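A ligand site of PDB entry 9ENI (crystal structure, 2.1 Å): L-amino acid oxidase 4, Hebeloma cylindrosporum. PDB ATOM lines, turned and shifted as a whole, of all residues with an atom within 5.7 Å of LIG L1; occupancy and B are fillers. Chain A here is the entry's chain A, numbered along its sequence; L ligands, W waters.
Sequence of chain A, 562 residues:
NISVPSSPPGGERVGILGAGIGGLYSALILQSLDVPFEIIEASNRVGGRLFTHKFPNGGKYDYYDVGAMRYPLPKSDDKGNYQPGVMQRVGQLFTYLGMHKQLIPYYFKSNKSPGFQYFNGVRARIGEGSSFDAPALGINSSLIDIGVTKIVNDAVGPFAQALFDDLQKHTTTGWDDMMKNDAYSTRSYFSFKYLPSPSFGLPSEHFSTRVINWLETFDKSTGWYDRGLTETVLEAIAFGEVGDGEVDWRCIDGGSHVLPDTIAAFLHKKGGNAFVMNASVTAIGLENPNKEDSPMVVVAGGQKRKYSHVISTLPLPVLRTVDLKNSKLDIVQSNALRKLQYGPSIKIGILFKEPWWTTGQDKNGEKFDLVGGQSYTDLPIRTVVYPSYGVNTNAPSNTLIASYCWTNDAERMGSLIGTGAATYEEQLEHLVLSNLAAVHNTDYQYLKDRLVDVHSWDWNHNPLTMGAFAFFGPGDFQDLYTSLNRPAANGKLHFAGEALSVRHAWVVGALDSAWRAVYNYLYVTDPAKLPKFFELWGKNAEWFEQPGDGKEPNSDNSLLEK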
ATOM      1  N   MET A  69     -18.388  14.246 -13.651  1.00  0.00           N
ATOM      2  CA  MET A  69     -18.419  15.353 -14.602  1.00  0.00           C
ATOM      3  C   MET A  69     -19.392  16.478 -14.245  1.00  0.00           C
ATOM      4  O   MET A  69     -19.262  17.560 -14.820  1.00  0.00           O
ATOM      5  CB  MET A  69     -18.772  14.858 -16.009  1.00  0.00           C
ATOM      6  CG  MET A  69     -20.222  14.418 -16.179  1.00  0.00           C
ATOM      7  SD  MET A  69     -20.591  13.799 -17.838  1.00  0.00           S
ATOM      8  CE  MET A  69     -22.341  13.470 -17.710  1.00  0.00           C
ATOM      9  N   ARG A  70     -20.340  16.287 -13.327  1.00  0.00           N
ATOM     10  CA  ARG A  70     -21.359  17.292 -13.068  1.00  0.00           C
ATOM     11  C   ARG A  70     -21.713  17.281 -11.591  1.00  0.00           C
ATOM     12  O   ARG A  70     -21.763  16.223 -10.964  1.00  0.00           O
ATOM     13  CB  ARG A  70     -22.625  17.037 -13.899  1.00  0.00           C
ATOM     14  CG  ARG A  70     -23.243  15.675 -13.672  1.00  0.00           C
ATOM     15  CD  ARG A  70     -24.323  15.381 -14.698  1.00  0.00           C
ATOM     16  NE  ARG A  70     -24.818  14.015 -14.613  1.00  0.00           N
ATOM     17  CZ  ARG A  70     -25.602  13.437 -15.512  1.00  0.00           C
ATOM     18  NH1 ARG A  70     -25.997  14.078 -16.597  1.00  0.00           N
ATOM     19  NH2 ARG A  70     -26.004  12.185 -15.314  1.00  0.00           N
ATOM     20  N   TRP A 224     -32.515  -0.718 -13.660  1.00  0.00           N
ATOM     21  CA  TRP A 224     -32.407   0.129 -12.481  1.00  0.00           C
ATOM     22  C   TRP A 224     -33.416  -0.260 -11.413  1.00  0.00           C
ATOM     23  O   TRP A 224     -33.107  -0.293 -10.219  1.00  0.00           O
ATOM     24  CB  TRP A 224     -32.591   1.592 -12.890  1.00  0.00           C
ATOM     25  CG  TRP A 224     -32.503   2.604 -11.767  1.00  0.00           C
ATOM     26  CD1 TRP A 224     -33.352   2.736 -10.712  1.00  0.00           C
ATOM     27  CD2 TRP A 224     -31.517   3.627 -11.612  1.00  0.00           C
ATOM     28  NE1 TRP A 224     -32.958   3.773  -9.907  1.00  0.00           N
ATOM     29  CE2 TRP A 224     -31.825   4.335 -10.439  1.00  0.00           C
ATOM     30  CE3 TRP A 224     -30.397   4.016 -12.362  1.00  0.00           C
ATOM     31  CZ2 TRP A 224     -31.065   5.410  -9.987  1.00  0.00           C
ATOM     32  CZ3 TRP A 224     -29.633   5.080 -11.903  1.00  0.00           C
ATOM     33  CH2 TRP A 224     -29.974   5.760 -10.728  1.00  0.00           C
ATOM     34  N   GLU A 235     -31.167   8.817  -5.004  1.00  0.00           N
ATOM     35  CA  GLU A 235     -30.767   9.483  -6.239  1.00  0.00           C
ATOM     36  C   GLU A 235     -31.639  10.702  -6.512  1.00  0.00           C
ATOM     37  O   GLU A 235     -31.137  11.744  -6.938  1.00  0.00           O
ATOM     38  CB  GLU A 235     -30.818   8.509  -7.413  1.00  0.00           C
ATOM     39  CG  GLU A 235     -30.365   9.106  -8.736  1.00  0.00           C
ATOM     40  CD  GLU A 235     -31.501   9.742  -9.530  1.00  0.00           C
ATOM     41  OE1 GLU A 235     -32.632   9.847  -9.005  1.00  0.00           O
ATOM     42  OE2 GLU A 235     -31.265  10.151 -10.684  1.00  0.00           O
ATOM     43  N   PHE A 239     -30.209  14.558  -7.033  1.00  0.00           N
ATOM     44  CA  PHE A 239     -30.502  15.361  -8.206  1.00  0.00           C
ATOM     45  C   PHE A 239     -31.331  16.603  -7.878  1.00  0.00           C
ATOM     46  O   PHE A 239     -31.673  17.361  -8.797  1.00  0.00           O
ATOM     47  CB  PHE A 239     -31.230  14.511  -9.258  1.00  0.00           C
ATOM     48  CG  PHE A 239     -30.293  13.750 -10.161  1.00  0.00           C
ATOM     49  CD1 PHE A 239     -29.760  12.533  -9.750  1.00  0.00           C
ATOM     50  CD2 PHE A 239     -29.949  14.238 -11.403  1.00  0.00           C
ATOM     51  CE1 PHE A 239     -28.896  11.825 -10.580  1.00  0.00           C
ATOM     52  CE2 PHE A 239     -29.084  13.540 -12.231  1.00  0.00           C
ATOM     53  CZ  PHE A 239     -28.565  12.334 -11.820  1.00  0.00           C
ATOM     54  N   TRP A 249     -26.191  23.506 -11.158  1.00  0.00           N
ATOM     55  CA  TRP A 249     -25.381  22.496 -11.832  1.00  0.00           C
ATOM     56  C   TRP A 249     -24.062  23.117 -12.277  1.00  0.00           C
ATOM     57  O   TRP A 249     -24.061  24.109 -13.021  1.00  0.00           O
ATOM     58  CB  TRP A 249     -26.128  21.910 -13.026  1.00  0.00           C
ATOM     59  CG  TRP A 249     -27.173  20.905 -12.662  1.00  0.00           C
ATOM     60  CD1 TRP A 249     -28.516  21.120 -12.568  1.00  0.00           C
ATOM     61  CD2 TRP A 249     -26.971  19.526 -12.330  1.00  0.00           C
ATOM     62  NE1 TRP A 249     -29.155  19.970 -12.213  1.00  0.00           N
ATOM     63  CE2 TRP A 249     -28.239  18.976 -12.060  1.00  0.00           C
ATOM     64  CE3 TRP A 249     -25.846  18.701 -12.248  1.00  0.00           C
ATOM     65  CZ2 TRP A 249     -28.407  17.634 -11.708  1.00  0.00           C
ATOM     66  CZ3 TRP A 249     -26.019  17.371 -11.902  1.00  0.00           C
ATOM     67  CH2 TRP A 249     -27.290  16.852 -11.635  1.00  0.00           C
ATOM     68  N   TYR A 404     -23.457   7.140 -22.593  1.00  0.00           N
ATOM     69  CA  TYR A 404     -23.238   7.058 -21.156  1.00  0.00           C
ATOM     70  C   TYR A 404     -24.334   6.147 -20.625  1.00  0.00           C
ATOM     71  O   TYR A 404     -25.505   6.526 -20.604  1.00  0.00           O
ATOM     72  CB  TYR A 404     -23.277   8.450 -20.516  1.00  0.00           C
ATOM     73  CG  TYR A 404     -23.184   8.467 -19.009  1.00  0.00           C
ATOM     74  CD1 TYR A 404     -22.610   7.414 -18.302  1.00  0.00           C
ATOM     75  CD2 TYR A 404     -23.691   9.544 -18.285  1.00  0.00           C
ATOM     76  CE1 TYR A 404     -22.536   7.435 -16.916  1.00  0.00           C
ATOM     77  CE2 TYR A 404     -23.631   9.567 -16.901  1.00  0.00           C
ATOM     78  CZ  TYR A 404     -23.051   8.519 -16.222  1.00  0.00           C
ATOM     79  OH  TYR A 404     -22.991   8.542 -14.838  1.00  0.00           O
ATOM     80  N   TRP A 406     -25.860   2.886 -17.912  1.00  0.00           N
ATOM     81  CA  TRP A 406     -25.944   2.279 -16.590  1.00  0.00           C
ATOM     82  C   TRP A 406     -26.486   0.855 -16.709  1.00  0.00           C
ATOM     83  O   TRP A 406     -26.951   0.425 -17.769  1.00  0.00           O
ATOM     84  CB  TRP A 406     -26.858   3.095 -15.664  1.00  0.00           C
ATOM     85  CG  TRP A 406     -26.399   4.498 -15.397  1.00  0.00           C
ATOM     86  CD1 TRP A 406     -25.116   4.935 -15.302  1.00  0.00           C
ATOM     87  CD2 TRP A 406     -27.231   5.641 -15.190  1.00  0.00           C
ATOM     88  NE1 TRP A 406     -25.091   6.283 -15.045  1.00  0.00           N
ATOM     89  CE2 TRP A 406     -26.385   6.744 -14.971  1.00  0.00           C
ATOM     90  CE3 TRP A 406     -28.620   5.843 -15.168  1.00  0.00           C
ATOM     91  CZ2 TRP A 406     -26.872   8.027 -14.736  1.00  0.00           C
ATOM     92  CZ3 TRP A 406     -29.096   7.122 -14.916  1.00  0.00           C
ATOM     93  CH2 TRP A 406     -28.227   8.197 -14.719  1.00  0.00           C
ATOM     94  N   PHE A 469     -19.576   2.064  -9.341  1.00  0.00           N
ATOM     95  CA  PHE A 469     -19.829   2.627  -8.021  1.00  0.00           C
ATOM     96  C   PHE A 469     -20.805   1.727  -7.285  1.00  0.00           C
ATOM     97  O   PHE A 469     -21.424   0.826  -7.859  1.00  0.00           O
ATOM     98  CB  PHE A 469     -20.364   4.057  -8.108  1.00  0.00           C
ATOM     99  CG  PHE A 469     -21.214   4.314  -9.331  1.00  0.00           C
ATOM    100  CD1 PHE A 469     -22.407   3.622  -9.525  1.00  0.00           C
ATOM    101  CD2 PHE A 469     -20.810   5.231 -10.286  1.00  0.00           C
ATOM    102  CE1 PHE A 469     -23.178   3.852 -10.647  1.00  0.00           C
ATOM    103  CE2 PHE A 469     -21.582   5.462 -11.408  1.00  0.00           C
ATOM    104  CZ  PHE A 469     -22.760   4.778 -11.597  1.00  0.00           C
ATOM    105  N   HIS A 504     -24.137   7.336  -3.004  1.00  0.00           N
ATOM    106  CA  HIS A 504     -23.397   6.506  -3.941  1.00  0.00           C
ATOM    107  C   HIS A 504     -23.347   7.166  -5.313  1.00  0.00           C
ATOM    108  O   HIS A 504     -24.293   7.837  -5.735  1.00  0.00           O
ATOM    109  CB  HIS A 504     -24.046   5.118  -4.042  1.00  0.00           C
ATOM    110  CG  HIS A 504     -23.962   4.322  -2.767  1.00  0.00           C
ATOM    111  ND1 HIS A 504     -24.863   3.335  -2.456  1.00  0.00           N
ATOM    112  CD2 HIS A 504     -23.071   4.359  -1.755  1.00  0.00           C
ATOM    113  CE1 HIS A 504     -24.538   2.796  -1.288  1.00  0.00           C
ATOM    114  NE2 HIS A 504     -23.450   3.396  -0.839  1.00  0.00           N
ATOM    115  N   ALA A 505     -22.233   6.961  -5.999  1.00  0.00           N
ATOM    116  CA  ALA A 505     -22.037   7.484  -7.355  1.00  0.00           C
ATOM    117  C   ALA A 505     -21.957   9.003  -7.373  1.00  0.00           C
ATOM    118  O   ALA A 505     -22.241   9.644  -8.396  1.00  0.00           O
ATOM    119  CB  ALA A 505     -23.141   7.002  -8.301  1.00  0.00           C
ATOM    120  N   TRP A 506     -21.556   9.601  -6.253  1.00  0.00           N
ATOM    121  CA  TRP A 506     -21.337  11.035  -6.152  1.00  0.00           C
ATOM    122  C   TRP A 506     -20.036  11.296  -5.415  1.00  0.00           C
ATOM    123  O   TRP A 506     -19.622  10.511  -4.549  1.00  0.00           O
ATOM    124  CB  TRP A 506     -22.479  11.744  -5.420  1.00  0.00           C
ATOM    125  CG  TRP A 506     -23.787  11.719  -6.155  1.00  0.00           C
ATOM    126  CD1 TRP A 506     -24.862  10.927  -5.877  1.00  0.00           C
ATOM    127  CD2 TRP A 506     -24.156  12.519  -7.279  1.00  0.00           C
ATOM    128  NE1 TRP A 506     -25.882  11.182  -6.756  1.00  0.00           N
ATOM    129  CE2 TRP A 506     -25.474  12.154  -7.627  1.00  0.00           C
ATOM    130  CE3 TRP A 506     -23.507  13.501  -8.036  1.00  0.00           C
ATOM    131  CZ2 TRP A 506     -26.154  12.745  -8.695  1.00  0.00           C
ATOM    132  CZ3 TRP A 506     -24.178  14.078  -9.090  1.00  0.00           C
ATOM    133  CH2 TRP A 506     -25.488  13.707  -9.408  1.00  0.00           C
HETATM  134  N1  LIG L   1     -23.989  10.399 -10.384  1.00  0.00           N
HETATM  135  C1  LIG L   1     -24.079   9.925 -11.751  1.00  0.00           C
HETATM  136  C2  LIG L   1     -24.238  11.095 -12.712  1.00  0.00           C
HETATM  137  O1  LIG L   1     -25.031  12.005 -12.478  1.00  0.00           O
HETATM  138  C3  LIG L   1     -25.250   8.960 -11.966  1.00  0.00           C
HETATM  139  C4  LIG L   1     -25.341   7.820 -11.003  1.00  0.00           C
HETATM  140  C5  LIG L   1     -26.152   8.173  -9.783  1.00  0.00           C
HETATM  141  O2  LIG L   1     -26.201   9.334  -9.377  1.00  0.00           O
HETATM  142  N2  LIG L   1     -26.804   7.173  -9.199  1.00  0.00           N
HETATM  143  O3  LIG L   1     -23.671  11.097 -13.806  1.00  0.00           O
HETATM  144  P1  LG2 L   2     -11.864   6.114  -6.221  1.00  0.00           P
HETATM  145  O1  LG2 L   2     -12.101   4.817  -6.912  1.00  0.00           O
HETATM  146  O2  LG2 L   2     -12.035   7.381  -6.992  1.00  0.00           O
HETATM  147  O3  LG2 L   2     -10.392   6.091  -5.569  1.00  0.00           O
HETATM  148  C1  LG2 L   2      -9.834   4.847  -5.083  1.00  0.00           C
HETATM  149  C2  LG2 L   2      -8.338   4.863  -5.330  1.00  0.00           C
HETATM  150  O4  LG2 L   2      -7.764   3.607  -4.895  1.00  0.00           O
HETATM  151  C3  LG2 L   2      -7.909   5.029  -6.793  1.00  0.00           C
HETATM  152  O5  LG2 L   2      -6.861   5.978  -6.917  1.00  0.00           O
HETATM  153  C4  LG2 L   2      -7.407   3.631  -7.177  1.00  0.00           C
HETATM  154  O6  LG2 L   2      -6.454   3.653  -8.226  1.00  0.00           O
HETATM  155  C5  LG2 L   2      -6.819   3.173  -5.856  1.00  0.00           C
HETATM  156  N1  LG2 L   2      -6.663   1.738  -5.691  1.00  0.00           N
HETATM  157  C6  LG2 L   2      -7.458   0.733  -6.176  1.00  0.00           C
HETATM  158  N2  LG2 L   2      -7.044  -0.465  -5.817  1.00  0.00           N
HETATM  159  C7  LG2 L   2      -5.904  -0.227  -5.053  1.00  0.00           C
HETATM  160  C8  LG2 L   2      -5.008  -1.084  -4.388  1.00  0.00           C
HETATM  161  N3  LG2 L   2      -5.129  -2.406  -4.367  1.00  0.00           N
HETATM  162  N4  LG2 L   2      -3.985  -0.513  -3.709  1.00  0.00           N
HETATM  163  C9  LG2 L   2      -3.884   0.830  -3.723  1.00  0.00           C
HETATM  164  N5  LG2 L   2      -4.660   1.724  -4.311  1.00  0.00           N
HETATM  165  C10 LG2 L   2      -5.669   1.127  -4.969  1.00  0.00           C
HETATM  166  N6  LG2 L   2     -19.704  11.922  -8.949  1.00  0.00           N
HETATM  167  C11 LG2 L   2     -20.148  13.215  -8.997  1.00  0.00           C
HETATM  168  O7  LG2 L   2     -20.067  13.938  -8.014  1.00  0.00           O
HETATM  169  N7  LG2 L   2     -20.663  13.652 -10.187  1.00  0.00           N
HETATM  170  C12 LG2 L   2     -20.788  12.893 -11.333  1.00  0.00           C
HETATM  171  O8  LG2 L   2     -21.264  13.395 -12.349  1.00  0.00           O
HETATM  172  C13 LG2 L   2     -20.339  11.564 -11.261  1.00  0.00           C
HETATM  173  N8  LG2 L   2     -20.415  10.726 -12.336  1.00  0.00           N
HETATM  174  C14 LG2 L   2     -19.759   9.511 -12.360  1.00  0.00           C
HETATM  175  C15 LG2 L   2     -19.650   8.788 -13.528  1.00  0.00           C
HETATM  176  C16 LG2 L   2     -18.981   7.596 -13.567  1.00  0.00           C
HETATM  177  C17 LG2 L   2     -18.890   6.826 -14.857  1.00  0.00           C
HETATM  178  C18 LG2 L   2     -18.383   7.088 -12.363  1.00  0.00           C
HETATM  179  C19 LG2 L   2     -17.640   5.781 -12.369  1.00  0.00           C
HETATM  180  C20 LG2 L   2     -18.484   7.811 -11.200  1.00  0.00           C
HETATM  181  C21 LG2 L   2     -19.175   9.029 -11.176  1.00  0.00           C
HETATM  182  N9  LG2 L   2     -19.315   9.790  -9.979  1.00  0.00           N
HETATM  183  C22 LG2 L   2     -19.783  11.088 -10.046  1.00  0.00           C
HETATM  184  C23 LG2 L   2     -18.935   9.209  -8.674  1.00  0.00           C
HETATM  185  C24 LG2 L   2     -17.545   9.635  -8.248  1.00  0.00           C
HETATM  186  O9  LG2 L   2     -16.675   9.617  -9.374  1.00  0.00           O
HETATM  187  C25 LG2 L   2     -17.055   8.653  -7.188  1.00  0.00           C
HETATM  188  O10 LG2 L   2     -18.103   8.431  -6.224  1.00  0.00           O
HETATM  189  C26 LG2 L   2     -15.816   9.117  -6.421  1.00  0.00           C
HETATM  190  O11 LG2 L   2     -14.871   9.683  -7.318  1.00  0.00           O
HETATM  191  C27 LG2 L   2     -15.182   7.961  -5.683  1.00  0.00           C
HETATM  192  O12 LG2 L   2     -14.015   8.385  -4.939  1.00  0.00           O
HETATM  193  P2  LG2 L   2     -13.324   7.347  -3.940  1.00  0.00           P
HETATM  194  O13 LG2 L   2     -12.149   8.041  -3.330  1.00  0.00           O
HETATM  195  O14 LG2 L   2     -14.406   6.781  -3.088  1.00  0.00           O
HETATM  196  O15 LG2 L   2     -12.831   6.190  -4.930  1.00  0.00           O
HETATM  197  O   HOH W   1     -26.870   4.535  -9.639  1.00  0.00           O
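The backbone carbonyl oxygen of Arg 70 is in hydrogen-bond range of a nitrogen (N7) of LG2 L2, at 2.9 Å. A nitrogen (N6) of LG2 L2 sits close to the backbone carbonyl oxygen (O) of Ala 505 (3.5 Å). The backbone NH (N) of Met 69 sits at hydrogen-bond distance from an oxygen (O8) of LG2 L2 (3.3 Å). The guanidinium group (NE) of Arg 70 lies within salt-bridge range of an oxygen (O1) of LIG L1 (2.9 Å). The backbone NH (N) of Arg 70 lies within hydrogen-bond range of an oxygen (O8) of LG2 L2, 3.2 Å away. A nitrogen (N1) of LIG L1 lies within hydrogen-bond range of the backbone carbonyl oxygen (O) of Ala 505. The backbone carbonyl oxygen of Trp 506 is in hydrogen-bond range of an oxygen (O10) of LG2 L2 (3.1 Å). The side-chain hydroxyl (OH) of Tyr 404 sits at hydrogen-bond distance from an oxygen (O3) of LIG L1, at 2.8 Å. NE1 of Trp 506 is in hydrogen-bond range of O2 of LIG L1 (3.2 Å).
The indole nitrogen of Trp 406 is in hydrogen-bond range of the side-chain hydroxyl of Tyr 404, 3.1 Å away.
Trp 224 touches LIG L1 (CH2 to N2, 3.8 Å). Phe 239 touches LIG L1 (CZ to O1, 3.6 Å). CZ2 of Trp 406 touches C3 of LIG L1, at 3.3 Å. Hydrophobic or aromatic side chains that line LIG L1: Trp 224, Phe 239, Tyr 404, Trp 406, Ala 505 and Trp 506. The nearest printed residue that does not touch LIG L1 is Phe 469 (4.03 Å).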
